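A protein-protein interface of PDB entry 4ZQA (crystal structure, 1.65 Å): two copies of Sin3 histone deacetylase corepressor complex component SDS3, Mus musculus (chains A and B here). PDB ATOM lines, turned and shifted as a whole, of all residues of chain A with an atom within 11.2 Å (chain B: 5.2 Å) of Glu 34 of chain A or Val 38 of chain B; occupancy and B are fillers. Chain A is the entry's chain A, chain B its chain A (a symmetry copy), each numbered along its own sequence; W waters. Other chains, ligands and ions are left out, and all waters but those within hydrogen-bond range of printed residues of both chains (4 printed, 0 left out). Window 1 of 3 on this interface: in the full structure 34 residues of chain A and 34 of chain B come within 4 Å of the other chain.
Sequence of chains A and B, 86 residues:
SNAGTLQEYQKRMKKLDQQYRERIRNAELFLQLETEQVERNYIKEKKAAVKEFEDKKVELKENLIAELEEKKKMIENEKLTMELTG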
ATOM      1  N   ARG A  25     -23.560  -5.886 -16.561  1.00  0.00           N
ATOM      2  CA  ARG A  25     -24.327  -4.653 -16.765  1.00  0.00           C
ATOM      3  C   ARG A  25     -24.486  -3.849 -15.467  1.00  0.00           C
ATOM      4  O   ARG A  25     -24.272  -2.611 -15.438  1.00  0.00           O
ATOM      5  CB  ARG A  25     -25.702  -5.061 -17.307  1.00  0.00           C
ATOM      6  CG  ARG A  25     -26.541  -3.996 -17.909  1.00  0.00           C
ATOM      7  CD  ARG A  25     -27.757  -4.635 -18.580  1.00  0.00           C
ATOM      8  NE  ARG A  25     -27.403  -5.468 -19.728  1.00  0.00           N
ATOM      9  CZ  ARG A  25     -27.649  -6.782 -19.862  1.00  0.00           C
ATOM     10  NH1 ARG A  25     -28.238  -7.487 -18.914  1.00  0.00           N
ATOM     11  NH2 ARG A  25     -27.265  -7.417 -20.971  1.00  0.00           N
ATOM     12  N   ASN A  26     -24.888  -4.530 -14.407  1.00  0.00           N
ATOM     13  CA  ASN A  26     -25.015  -3.900 -13.081  1.00  0.00           C
ATOM     14  C   ASN A  26     -23.686  -3.325 -12.580  1.00  0.00           C
ATOM     15  O   ASN A  26     -23.655  -2.246 -11.991  1.00  0.00           O
ATOM     16  CB  ASN A  26     -25.620  -4.854 -12.059  1.00  0.00           C
ATOM     17  CG  ASN A  26     -27.118  -4.999 -12.244  1.00  0.00           C
ATOM     18  OD1 ASN A  26     -27.796  -4.026 -12.665  1.00  0.00           O
ATOM     19  ND2 ASN A  26     -27.665  -6.154 -11.872  1.00  0.00           N
ATOM     20  N   ALA A  27     -22.592  -4.020 -12.855  1.00  0.00           N
ATOM     21  CA  ALA A  27     -21.257  -3.482 -12.489  1.00  0.00           C
ATOM     22  C   ALA A  27     -20.945  -2.191 -13.207  1.00  0.00           C
ATOM     23  O   ALA A  27     -20.398  -1.285 -12.594  1.00  0.00           O
ATOM     24  CB  ALA A  27     -20.157  -4.494 -12.767  1.00  0.00           C
ATOM     25  N   GLU A  28     -21.269  -2.126 -14.505  1.00  0.00           N
ATOM     26  CA  GLU A  28     -21.048  -0.929 -15.309  1.00  0.00           C
ATOM     27  C   GLU A  28     -21.880   0.235 -14.757  1.00  0.00           C
ATOM     28  O   GLU A  28     -21.386   1.359 -14.603  1.00  0.00           O
ATOM     29  CB  GLU A  28     -21.404  -1.173 -16.779  1.00  0.00           C
ATOM     30  CG  GLU A  28     -20.540  -2.228 -17.501  1.00  0.00           C
ATOM     31  CD  GLU A  28     -21.176  -2.811 -18.776  1.00  0.00           C
ATOM     32  OE1 GLU A  28     -22.388  -2.571 -19.049  1.00  0.00           O
ATOM     33  OE2 GLU A  28     -20.459  -3.536 -19.513  1.00  0.00           O
ATOM     34  N   LEU A  29     -23.156  -0.029 -14.477  1.00  0.00           N
ATOM     35  CA  LEU A  29     -24.017   1.003 -13.916  1.00  0.00           C
ATOM     36  C   LEU A  29     -23.535   1.460 -12.523  1.00  0.00           C
ATOM     37  O   LEU A  29     -23.510   2.675 -12.210  1.00  0.00           O
ATOM     38  CB  LEU A  29     -25.493   0.511 -13.876  1.00  0.00           C
ATOM     39  CG  LEU A  29     -26.534   1.499 -13.318  1.00  0.00           C
ATOM     40  CD1 LEU A  29     -26.549   2.858 -14.053  1.00  0.00           C
ATOM     41  CD2 LEU A  29     -27.899   0.855 -13.389  1.00  0.00           C
ATOM     42  N   PHE A  30     -23.137   0.504 -11.695  1.00  0.00           N
ATOM     43  CA  PHE A  30     -22.660   0.806 -10.348  1.00  0.00           C
ATOM     44  C   PHE A  30     -21.408   1.670 -10.409  1.00  0.00           C
ATOM     45  O   PHE A  30     -21.286   2.610  -9.616  1.00  0.00           O
ATOM     46  CB  PHE A  30     -22.409  -0.482  -9.563  1.00  0.00           C
ATOM     47  CG  PHE A  30     -22.097  -0.277  -8.079  1.00  0.00           C
ATOM     48  CD1 PHE A  30     -23.102   0.024  -7.161  1.00  0.00           C
ATOM     49  CD2 PHE A  30     -20.804  -0.387  -7.604  1.00  0.00           C
ATOM     50  CE1 PHE A  30     -22.822   0.173  -5.822  1.00  0.00           C
ATOM     51  CE2 PHE A  30     -20.530  -0.238  -6.264  1.00  0.00           C
ATOM     52  CZ  PHE A  30     -21.532   0.066  -5.365  1.00  0.00           C
ATOM     53  N   LEU A  31     -20.534   1.387 -11.373  1.00  0.00           N
ATOM     54  CA  LEU A  31     -19.326   2.181 -11.606  1.00  0.00           C
ATOM     55  C   LEU A  31     -19.733   3.644 -11.849  1.00  0.00           C
ATOM     56  O   LEU A  31     -19.204   4.578 -11.206  1.00  0.00           O
ATOM     57  CB  LEU A  31     -18.558   1.621 -12.807  1.00  0.00           C
ATOM     58  CG  LEU A  31     -17.293   2.373 -13.303  1.00  0.00           C
ATOM     59  CD1 LEU A  31     -16.271   2.572 -12.209  1.00  0.00           C
ATOM     60  CD2 LEU A  31     -16.646   1.665 -14.480  1.00  0.00           C
ATOM     61  N   GLN A  32     -20.692   3.847 -12.754  1.00  0.00           N
ATOM     62  CA  GLN A  32     -21.129   5.210 -13.049  1.00  0.00           C
ATOM     63  C   GLN A  32     -21.747   5.932 -11.843  1.00  0.00           C
ATOM     64  O   GLN A  32     -21.478   7.097 -11.625  1.00  0.00           O
ATOM     65  CB  GLN A  32     -22.081   5.227 -14.216  1.00  0.00           C
ATOM     66  CG  GLN A  32     -21.433   4.719 -15.499  1.00  0.00           C
ATOM     67  CD  GLN A  32     -22.416   4.646 -16.588  1.00  0.00           C
ATOM     68  OE1 GLN A  32     -23.474   4.005 -16.429  1.00  0.00           O
ATOM     69  NE2 GLN A  32     -22.104   5.271 -17.726  1.00  0.00           N
ATOM     70  N   LEU A  33     -22.574   5.238 -11.064  1.00  0.00           N
ATOM     71  CA  LEU A  33     -23.173   5.853  -9.906  1.00  0.00           C
ATOM     72  C   LEU A  33     -22.156   6.125  -8.791  1.00  0.00           C
ATOM     73  O   LEU A  33     -22.203   7.166  -8.152  1.00  0.00           O
ATOM     74  CB  LEU A  33     -24.321   5.019  -9.378  1.00  0.00           C
ATOM     75  CG  LEU A  33     -25.433   4.790 -10.401  1.00  0.00           C
ATOM     76  CD1 LEU A  33     -26.372   3.713  -9.841  1.00  0.00           C
ATOM     77  CD2 LEU A  33     -26.150   6.080 -10.757  1.00  0.00           C
ATOM     78  N   GLU A  34     -21.248   5.197  -8.559  1.00  0.00           N
ATOM     79  CA  GLU A  34     -20.135   5.413  -7.623  1.00  0.00           C
ATOM     80  C   GLU A  34     -19.269   6.591  -8.024  1.00  0.00           C
ATOM     81  O   GLU A  34     -18.867   7.425  -7.180  1.00  0.00           O
ATOM     82  CB  GLU A  34     -19.265   4.164  -7.561  1.00  0.00           C
ATOM     83  CG  GLU A  34     -19.830   3.036  -6.710  1.00  0.00           C
ATOM     84  CD  GLU A  34     -19.507   3.157  -5.215  1.00  0.00           C
ATOM     85  OE1 GLU A  34     -18.494   2.525  -4.742  1.00  0.00           O
ATOM     86  OE2 GLU A  34     -20.293   3.859  -4.516  1.00  0.00           O
ATOM     87  N   THR A  35     -18.976   6.679  -9.312  1.00  0.00           N
ATOM     88  CA  THR A  35     -18.156   7.776  -9.836  1.00  0.00           C
ATOM     89  C   THR A  35     -18.862   9.099  -9.569  1.00  0.00           C
ATOM     90  O   THR A  35     -18.231  10.065  -9.150  1.00  0.00           O
ATOM     91  CB  THR A  35     -17.855   7.551 -11.341  1.00  0.00           C
ATOM     92  OG1 THR A  35     -17.031   6.364 -11.495  1.00  0.00           O
ATOM     93  CG2 THR A  35     -17.139   8.742 -11.968  1.00  0.00           C
ATOM     94  N   GLU A  36     -20.182   9.148  -9.800  1.00  0.00           N
ATOM     95  CA  GLU A  36     -20.925  10.387  -9.509  1.00  0.00           C
ATOM     96  C   GLU A  36     -20.850  10.765  -8.037  1.00  0.00           C
ATOM     97  O   GLU A  36     -20.759  11.975  -7.682  1.00  0.00           O
ATOM     98  CB  GLU A  36     -22.412  10.248  -9.950  1.00  0.00           C
ATOM     99  CG  GLU A  36     -23.258  11.470  -9.580  1.00  0.00           C
ATOM    100  CD  GLU A  36     -22.844  12.742 -10.313  1.00  0.00           C
ATOM    101  OE1 GLU A  36     -22.069  12.666 -11.302  1.00  0.00           O
ATOM    102  OE2 GLU A  36     -23.303  13.828  -9.897  1.00  0.00           O
ATOM    103  N   GLN A  37     -20.914   9.784  -7.152  1.00  0.00           N
ATOM    104  CA  GLN A  37     -20.830  10.073  -5.720  1.00  0.00           C
ATOM    105  C   GLN A  37     -19.452  10.642  -5.358  1.00  0.00           C
ATOM    106  O   GLN A  37     -19.355  11.623  -4.634  1.00  0.00           O
ATOM    107  CB  GLN A  37     -21.190   8.841  -4.872  1.00  0.00           C
ATOM    108  CG  GLN A  37     -21.257   9.093  -3.365  1.00  0.00           C
ATOM    109  CD  GLN A  37     -22.298  10.137  -2.928  1.00  0.00           C
ATOM    110  OE1 GLN A  37     -23.532   9.974  -3.120  1.00  0.00           O
ATOM    111  NE2 GLN A  37     -21.816  11.208  -2.305  1.00  0.00           N
ATOM    112  N   VAL A  38     -18.397  10.041  -5.887  1.00  0.00           N
ATOM    113  CA  VAL A  38     -17.029  10.575  -5.725  1.00  0.00           C
ATOM    114  C   VAL A  38     -16.928  12.053  -6.203  1.00  0.00           C
ATOM    115  O   VAL A  38     -16.325  12.907  -5.536  1.00  0.00           O
ATOM    116  CB  VAL A  38     -16.022   9.621  -6.440  1.00  0.00           C
ATOM    117  CG1 VAL A  38     -14.722  10.311  -6.686  1.00  0.00           C
ATOM    118  CG2 VAL A  38     -15.897   8.341  -5.628  1.00  0.00           C
ATOM    119  N   GLU A  39     -17.573  12.363  -7.322  1.00  0.00           N
ATOM    120  CA  GLU A  39     -17.604  13.742  -7.843  1.00  0.00           C
ATOM    121  C   GLU A  39     -18.368  14.682  -6.886  1.00  0.00           C
ATOM    122  O   GLU A  39     -17.904  15.811  -6.640  1.00  0.00           O
ATOM    123  CB  GLU A  39     -18.201  13.810  -9.270  1.00  0.00           C
ATOM    124  CG  GLU A  39     -17.411  13.080 -10.339  1.00  0.00           C
ATOM    125  CD  GLU A  39     -16.147  13.811 -10.821  1.00  0.00           C
ATOM    126  OE1 GLU A  39     -15.992  15.035 -10.555  1.00  0.00           O
ATOM    127  OE2 GLU A  39     -15.314  13.142 -11.490  1.00  0.00           O
ATOM    128  N   ARG A  40     -19.508  14.213  -6.350  1.00  0.00           N
ATOM    129  CA  ARG A  40     -20.289  14.996  -5.361  1.00  0.00           C
ATOM    130  C   ARG A  40     -19.448  15.298  -4.129  1.00  0.00           C
ATOM    131  O   ARG A  40     -19.483  16.397  -3.583  1.00  0.00           O
ATOM    132  CB  ARG A  40     -21.612  14.285  -4.958  1.00  0.00           C
ATOM    133  CG  ARG A  40     -22.674  14.397  -6.047  1.00  0.00           C
ATOM    134  CD  ARG A  40     -24.106  14.033  -5.594  1.00  0.00           C
ATOM    135  NE  ARG A  40     -24.166  12.623  -5.252  1.00  0.00           N
ATOM    136  CZ  ARG A  40     -24.602  11.631  -6.050  1.00  0.00           C
ATOM    137  NH1 ARG A  40     -25.124  11.873  -7.246  1.00  0.00           N
ATOM    138  NH2 ARG A  40     -24.549  10.362  -5.629  1.00  0.00           N
ATOM    139  N   ASN A  41     -18.667  14.317  -3.712  1.00  0.00           N
ATOM    140  CA  ASN A  41     -17.859  14.469  -2.511  1.00  0.00           C
ATOM    141  C   ASN A  41     -16.781  15.511  -2.709  1.00  0.00           C
ATOM    142  O   ASN A  41     -16.454  16.282  -1.779  1.00  0.00           O
ATOM    143  CB  ASN A  41     -17.237  13.151  -2.137  1.00  0.00           C
ATOM    144  CG  ASN A  41     -18.264  12.107  -1.718  1.00  0.00           C
ATOM    145  OD1 ASN A  41     -19.411  12.414  -1.369  1.00  0.00           O
ATOM    146  ND2 ASN A  41     -17.845  10.866  -1.738  1.00  0.00           N
ATOM    147  N   TYR A  42     -16.234  15.528  -3.928  1.00  0.00           N
ATOM    148  CA  TYR A  42     -15.243  16.526  -4.347  1.00  0.00           C
ATOM    149  C   TYR A  42     -15.845  17.946  -4.302  1.00  0.00           C
ATOM    150  O   TYR A  42     -15.273  18.861  -3.727  1.00  0.00           O
ATOM    151  CB  TYR A  42     -14.715  16.175  -5.734  1.00  0.00           C
ATOM    152  CG  TYR A  42     -13.903  17.251  -6.442  1.00  0.00           C
ATOM    153  CD1 TYR A  42     -12.697  17.703  -5.908  1.00  0.00           C
ATOM    154  CD2 TYR A  42     -14.307  17.762  -7.688  1.00  0.00           C
ATOM    155  CE1 TYR A  42     -11.922  18.645  -6.567  1.00  0.00           C
ATOM    156  CE2 TYR A  42     -13.542  18.710  -8.362  1.00  0.00           C
ATOM    157  CZ  TYR A  42     -12.341  19.149  -7.795  1.00  0.00           C
ATOM    158  OH  TYR A  42     -11.560  20.098  -8.437  1.00  0.00           O
ATOM    159  N   ILE A  43     -17.026  18.105  -4.894  1.00  0.00           N
ATOM    160  CA  ILE A  43     -17.722  19.407  -4.894  1.00  0.00           C
ATOM    161  C   ILE A  43     -17.999  19.890  -3.484  1.00  0.00           C
ATOM    162  O   ILE A  43     -17.807  21.071  -3.161  1.00  0.00           O
ATOM    163  CB  ILE A  43     -19.049  19.319  -5.698  1.00  0.00           C
ATOM    164  CG1 ILE A  43     -18.759  18.990  -7.159  1.00  0.00           C
ATOM    165  CG2 ILE A  43     -19.887  20.616  -5.582  1.00  0.00           C
ATOM    166  CD1 ILE A  43     -17.756  19.906  -7.852  1.00  0.00           C
ATOM    167  N   GLU B  34      -9.685   8.134  -5.233  1.00  0.00           N
ATOM    168  CA  GLU B  34     -11.018   7.537  -5.067  1.00  0.00           C
ATOM    169  C   GLU B  34     -11.546   6.944  -6.358  1.00  0.00           C
ATOM    170  O   GLU B  34     -12.112   5.827  -6.383  1.00  0.00           O
ATOM    171  CB  GLU B  34     -11.999   8.596  -4.577  1.00  0.00           C
ATOM    172  CG  GLU B  34     -11.901   8.916  -3.093  1.00  0.00           C
ATOM    173  CD  GLU B  34     -12.702   7.967  -2.192  1.00  0.00           C
ATOM    174  OE1 GLU B  34     -13.884   8.308  -1.822  1.00  0.00           O
ATOM    175  OE2 GLU B  34     -12.127   6.899  -1.833  1.00  0.00           O
ATOM    176  N   THR B  35     -11.364   7.677  -7.446  1.00  0.00           N
ATOM    177  CA  THR B  35     -11.816   7.217  -8.762  1.00  0.00           C
ATOM    178  C   THR B  35     -11.093   5.924  -9.114  1.00  0.00           C
ATOM    179  O   THR B  35     -11.710   4.981  -9.604  1.00  0.00           O
ATOM    180  CB  THR B  35     -11.605   8.329  -9.824  1.00  0.00           C
ATOM    181  OG1 THR B  35     -12.460   9.461  -9.511  1.00  0.00           O
ATOM    182  CG2 THR B  35     -11.913   7.842 -11.235  1.00  0.00           C
ATOM    183  N   GLU B  36      -9.779   5.864  -8.856  1.00  0.00           N
ATOM    184  CA  GLU B  36      -9.040   4.620  -9.128  1.00  0.00           C
ATOM    185  C   GLU B  36      -9.572   3.450  -8.312  1.00  0.00           C
ATOM    186  O   GLU B  36      -9.635   2.289  -8.808  1.00  0.00           O
ATOM    187  CB  GLU B  36      -7.520   4.815  -8.852  1.00  0.00           C
ATOM    188  CG  GLU B  36      -6.714   3.523  -9.020  1.00  0.00           C
ATOM    189  CD  GLU B  36      -6.695   3.001 -10.453  1.00  0.00           C
ATOM    190  OE1 GLU B  36      -7.085   3.743 -11.392  1.00  0.00           O
ATOM    191  OE2 GLU B  36      -6.282   1.835 -10.641  1.00  0.00           O
ATOM    192  N   GLN B  37      -9.934   3.693  -7.063  1.00  0.00           N
ATOM    193  CA  GLN B  37     -10.471   2.620  -6.227  1.00  0.00           C
ATOM    194  C   GLN B  37     -11.812   2.117  -6.778  1.00  0.00           C
ATOM    195  O   GLN B  37     -12.035   0.918  -6.871  1.00  0.00           O
ATOM    196  CB  GLN B  37     -10.576   3.050  -4.753  1.00  0.00           C
ATOM    197  CG  GLN B  37     -11.003   1.943  -3.788  1.00  0.00           C
ATOM    198  CD  GLN B  37     -10.060   0.730  -3.734  1.00  0.00           C
ATOM    199  OE1 GLN B  37      -8.864   0.827  -3.351  1.00  0.00           O
ATOM    200  NE2 GLN B  37     -10.596  -0.435  -4.088  1.00  0.00           N
ATOM    201  N   VAL B  38     -12.683   3.035  -7.167  1.00  0.00           N
ATOM    202  CA  VAL B  38     -13.950   2.678  -7.840  1.00  0.00           C
ATOM    203  C   VAL B  38     -13.702   1.802  -9.102  1.00  0.00           C
ATOM    204  O   VAL B  38     -14.392   0.798  -9.336  1.00  0.00           O
ATOM    205  CB  VAL B  38     -14.754   3.982  -8.137  1.00  0.00           C
ATOM    206  CG1 VAL B  38     -15.797   3.736  -9.174  1.00  0.00           C
ATOM    207  CG2 VAL B  38     -15.303   4.529  -6.827  1.00  0.00           C
ATOM    208  N   GLU B  39     -12.680   2.145  -9.876  1.00  0.00           N
ATOM    209  CA  GLU B  39     -12.306   1.358 -11.065  1.00  0.00           C
ATOM    210  C   GLU B  39     -11.813  -0.050 -10.669  1.00  0.00           C
ATOM    211  O   GLU B  39     -12.195  -1.038 -11.323  1.00  0.00           O
ATOM    212  CB  GLU B  39     -11.250   2.083 -11.935  1.00  0.00           C
ATOM    213  CG  GLU B  39     -11.704   3.395 -12.546  1.00  0.00           C
ATOM    214  CD  GLU B  39     -12.629   3.253 -13.768  1.00  0.00           C
ATOM    215  OE1 GLU B  39     -12.718   2.141 -14.358  1.00  0.00           O
ATOM    216  OE2 GLU B  39     -13.253   4.282 -14.141  1.00  0.00           O
ATOM    217  N   ARG B  40     -10.993  -0.133  -9.607  1.00  0.00           N
ATOM    218  CA  ARG B  40     -10.513  -1.438  -9.088  1.00  0.00           C
ATOM    219  C   ARG B  40     -11.685  -2.312  -8.665  1.00  0.00           C
ATOM    220  O   ARG B  40     -11.709  -3.514  -8.912  1.00  0.00           O
ATOM    221  CB  ARG B  40      -9.505  -1.271  -7.916  1.00  0.00           C
ATOM    222  CG  ARG B  40      -8.127  -0.838  -8.406  1.00  0.00           C
ATOM    223  CD  ARG B  40      -6.993  -0.989  -7.367  1.00  0.00           C
ATOM    224  NE  ARG B  40      -7.223  -0.081  -6.258  1.00  0.00           N
ATOM    225  CZ  ARG B  40      -6.660   1.130  -6.094  1.00  0.00           C
ATOM    226  NH1 ARG B  40      -5.733   1.590  -6.926  1.00  0.00           N
ATOM    227  NH2 ARG B  40      -7.006   1.894  -5.051  1.00  0.00           N
ATOM    228  N   ASN B  41     -12.672  -1.689  -8.047  1.00  0.00           N
ATOM    229  CA  ASN B  41     -13.821  -2.429  -7.545  1.00  0.00           C
ATOM    230  C   ASN B  41     -14.631  -3.009  -8.682  1.00  0.00           C
ATOM    231  O   ASN B  41     -15.165  -4.137  -8.580  1.00  0.00           O
ATOM    232  CB  ASN B  41     -14.686  -1.531  -6.703  1.00  0.00           C
ATOM    233  CG  ASN B  41     -13.998  -1.075  -5.422  1.00  0.00           C
ATOM    234  OD1 ASN B  41     -13.014  -1.663  -4.957  1.00  0.00           O
ATOM    235  ND2 ASN B  41     -14.530  -0.028  -4.841  1.00  0.00           N
ATOM    236  N   TYR B  42     -14.719  -2.230  -9.765  1.00  0.00           N
ATOM    237  CA  TYR B  42     -15.379  -2.655 -11.005  1.00  0.00           C
ATOM    238  C   TYR B  42     -14.664  -3.881 -11.612  1.00  0.00           C
ATOM    239  O   TYR B  42     -15.286  -4.882 -11.937  1.00  0.00           O
ATOM    240  CB  TYR B  42     -15.434  -1.487 -11.984  1.00  0.00           C
ATOM    241  CG  TYR B  42     -15.817  -1.823 -13.418  1.00  0.00           C
ATOM    242  CD1 TYR B  42     -17.071  -2.356 -13.716  1.00  0.00           C
ATOM    243  CD2 TYR B  42     -14.951  -1.533 -14.486  1.00  0.00           C
ATOM    244  CE1 TYR B  42     -17.453  -2.618 -15.023  1.00  0.00           C
ATOM    245  CE2 TYR B  42     -15.318  -1.792 -15.805  1.00  0.00           C
ATOM    246  CZ  TYR B  42     -16.579  -2.336 -16.069  1.00  0.00           C
ATOM    247  OH  TYR B  42     -16.972  -2.613 -17.370  1.00  0.00           O
HETATM  248  O   HOH W   1     -14.828  10.761  -2.112  1.00  0.00           O
HETATM  249  O   HOH W   2     -17.222   0.638  -6.090  1.00  0.00           O
HETATM  250  O   HOH W   3     -13.717  10.766 -11.379  1.00  0.00           O
HETATM  251  O   HOH W   4     -15.061   6.293 -13.194  1.00  0.00           O
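Of chain A, only Leu 31 (3.3 Å), Glu 34 (3.8 Å) and Thr 35 (3.7 Å) come within 4 Å of Val 38 of chain B.
Glu 34 of chain B touches just one residue of chain A: Val 38 (3.8 Å).
No residue of chain A comes within 4 Å of Gln 37 of chain B.
No residue of chain A comes within 4 Å of Arg 40 of chain B.
No residue of chain A comes within 4 Å of Asn 41 of chain B.
Of the printed residues of chain B, Ala 27 of chain A touches Tyr 42 (3.7 Å).
Of the printed residues of chain A, Tyr 42 of chain B touches Ala 27 (3.7 Å), Glu 28 (3.6 Å) and Leu 31 (3.6 Å).
Glu 36 of chain B touches none of the printed residues of chain A.
The nearest residue of chain A that does not touch Val 38 of chain B is Val 38 of chain A (4.04 Å).
Glu 34 of chain A touches Val 38 of chain B, and with the chains exchanged Val 38 of chain A touches Glu 34 of chain B.
Thr 35 of chain A touches Val 38 of chain B, and with the chains exchanged Val 38 of chain A touches Thr 35 of chain B.
Positions printed for both chains: 34, 35, 36, 37, 38, 39, 40, 41 and 42.
Of the 9 pairs that touch across the chains among the printed residues, 4 have their exchanged pair printed and touching as well.
Water W4 bridges the side-chain hydroxyl of Thr 35 of chain A (2.6 Å) and the side-chain carboxylate of Glu 39 of chain B (2.9 Å).
Water W3 bridges OG1 of Thr 35 of chain B (2.6 Å) and OE2 of Glu 39 of chain A (2.9 Å).
Water W2 bridges the side-chain carboxylate (OE1) of Glu 34 of chain A and the side-chain amide nitrogen (ND2) of Asn 41 of chain B.
Water W1 lies within hydrogen-bond range of the side-chain carboxylate (OE1) of Glu 34 of chain B (2.6 Å) and the side-chain amide nitrogen (ND2) of Asn 41 of chain A (3.0 Å).
O of Ala 27 of chain A touches CD1 of Tyr 42 of chain B, 3.7 Å away.
CG of Glu 28 of chain A touches OH of Tyr 42 of chain B, at 3.6 Å.
Leu 31 of chain A touches Val 38 of chain B (CD1 to CG1, 3.3 Å).
Glu 39 of chain B touches Leu 31 of chain A (OE1 to CD2, 3.96 Å).
Leu 31 of chain A touches Tyr 42 of chain B.
Val 38 of chain B touches Glu 34 of chain A.
OG1 of Thr 35 of chain A touches CG1 of Val 38 of chain B (3.7 Å).
CG1 of Val 38 of chain A touches CB of Glu 34 of chain B (3.8 Å).
Val 38 of chain A touches Thr 35 of chain B (CG1 to OG1, 3.7 Å).
O of Leu 31 of chain A is in hydrogen-bond range of OG1 of Thr 35 of chain A (2.8 Å).
Printed residues of chain A that touch a printed residue of chain B: Ala 27, Glu 28, Leu 31, Glu 34, Thr 35 and Val 38.
Of the 9 printed residues of chain B, 5 touch a printed residue of chain A.
Among the printed residues, no Asp or Glu carboxylate lies within 4 Å of a Lys or Arg side-chain nitrogen of the other chain.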
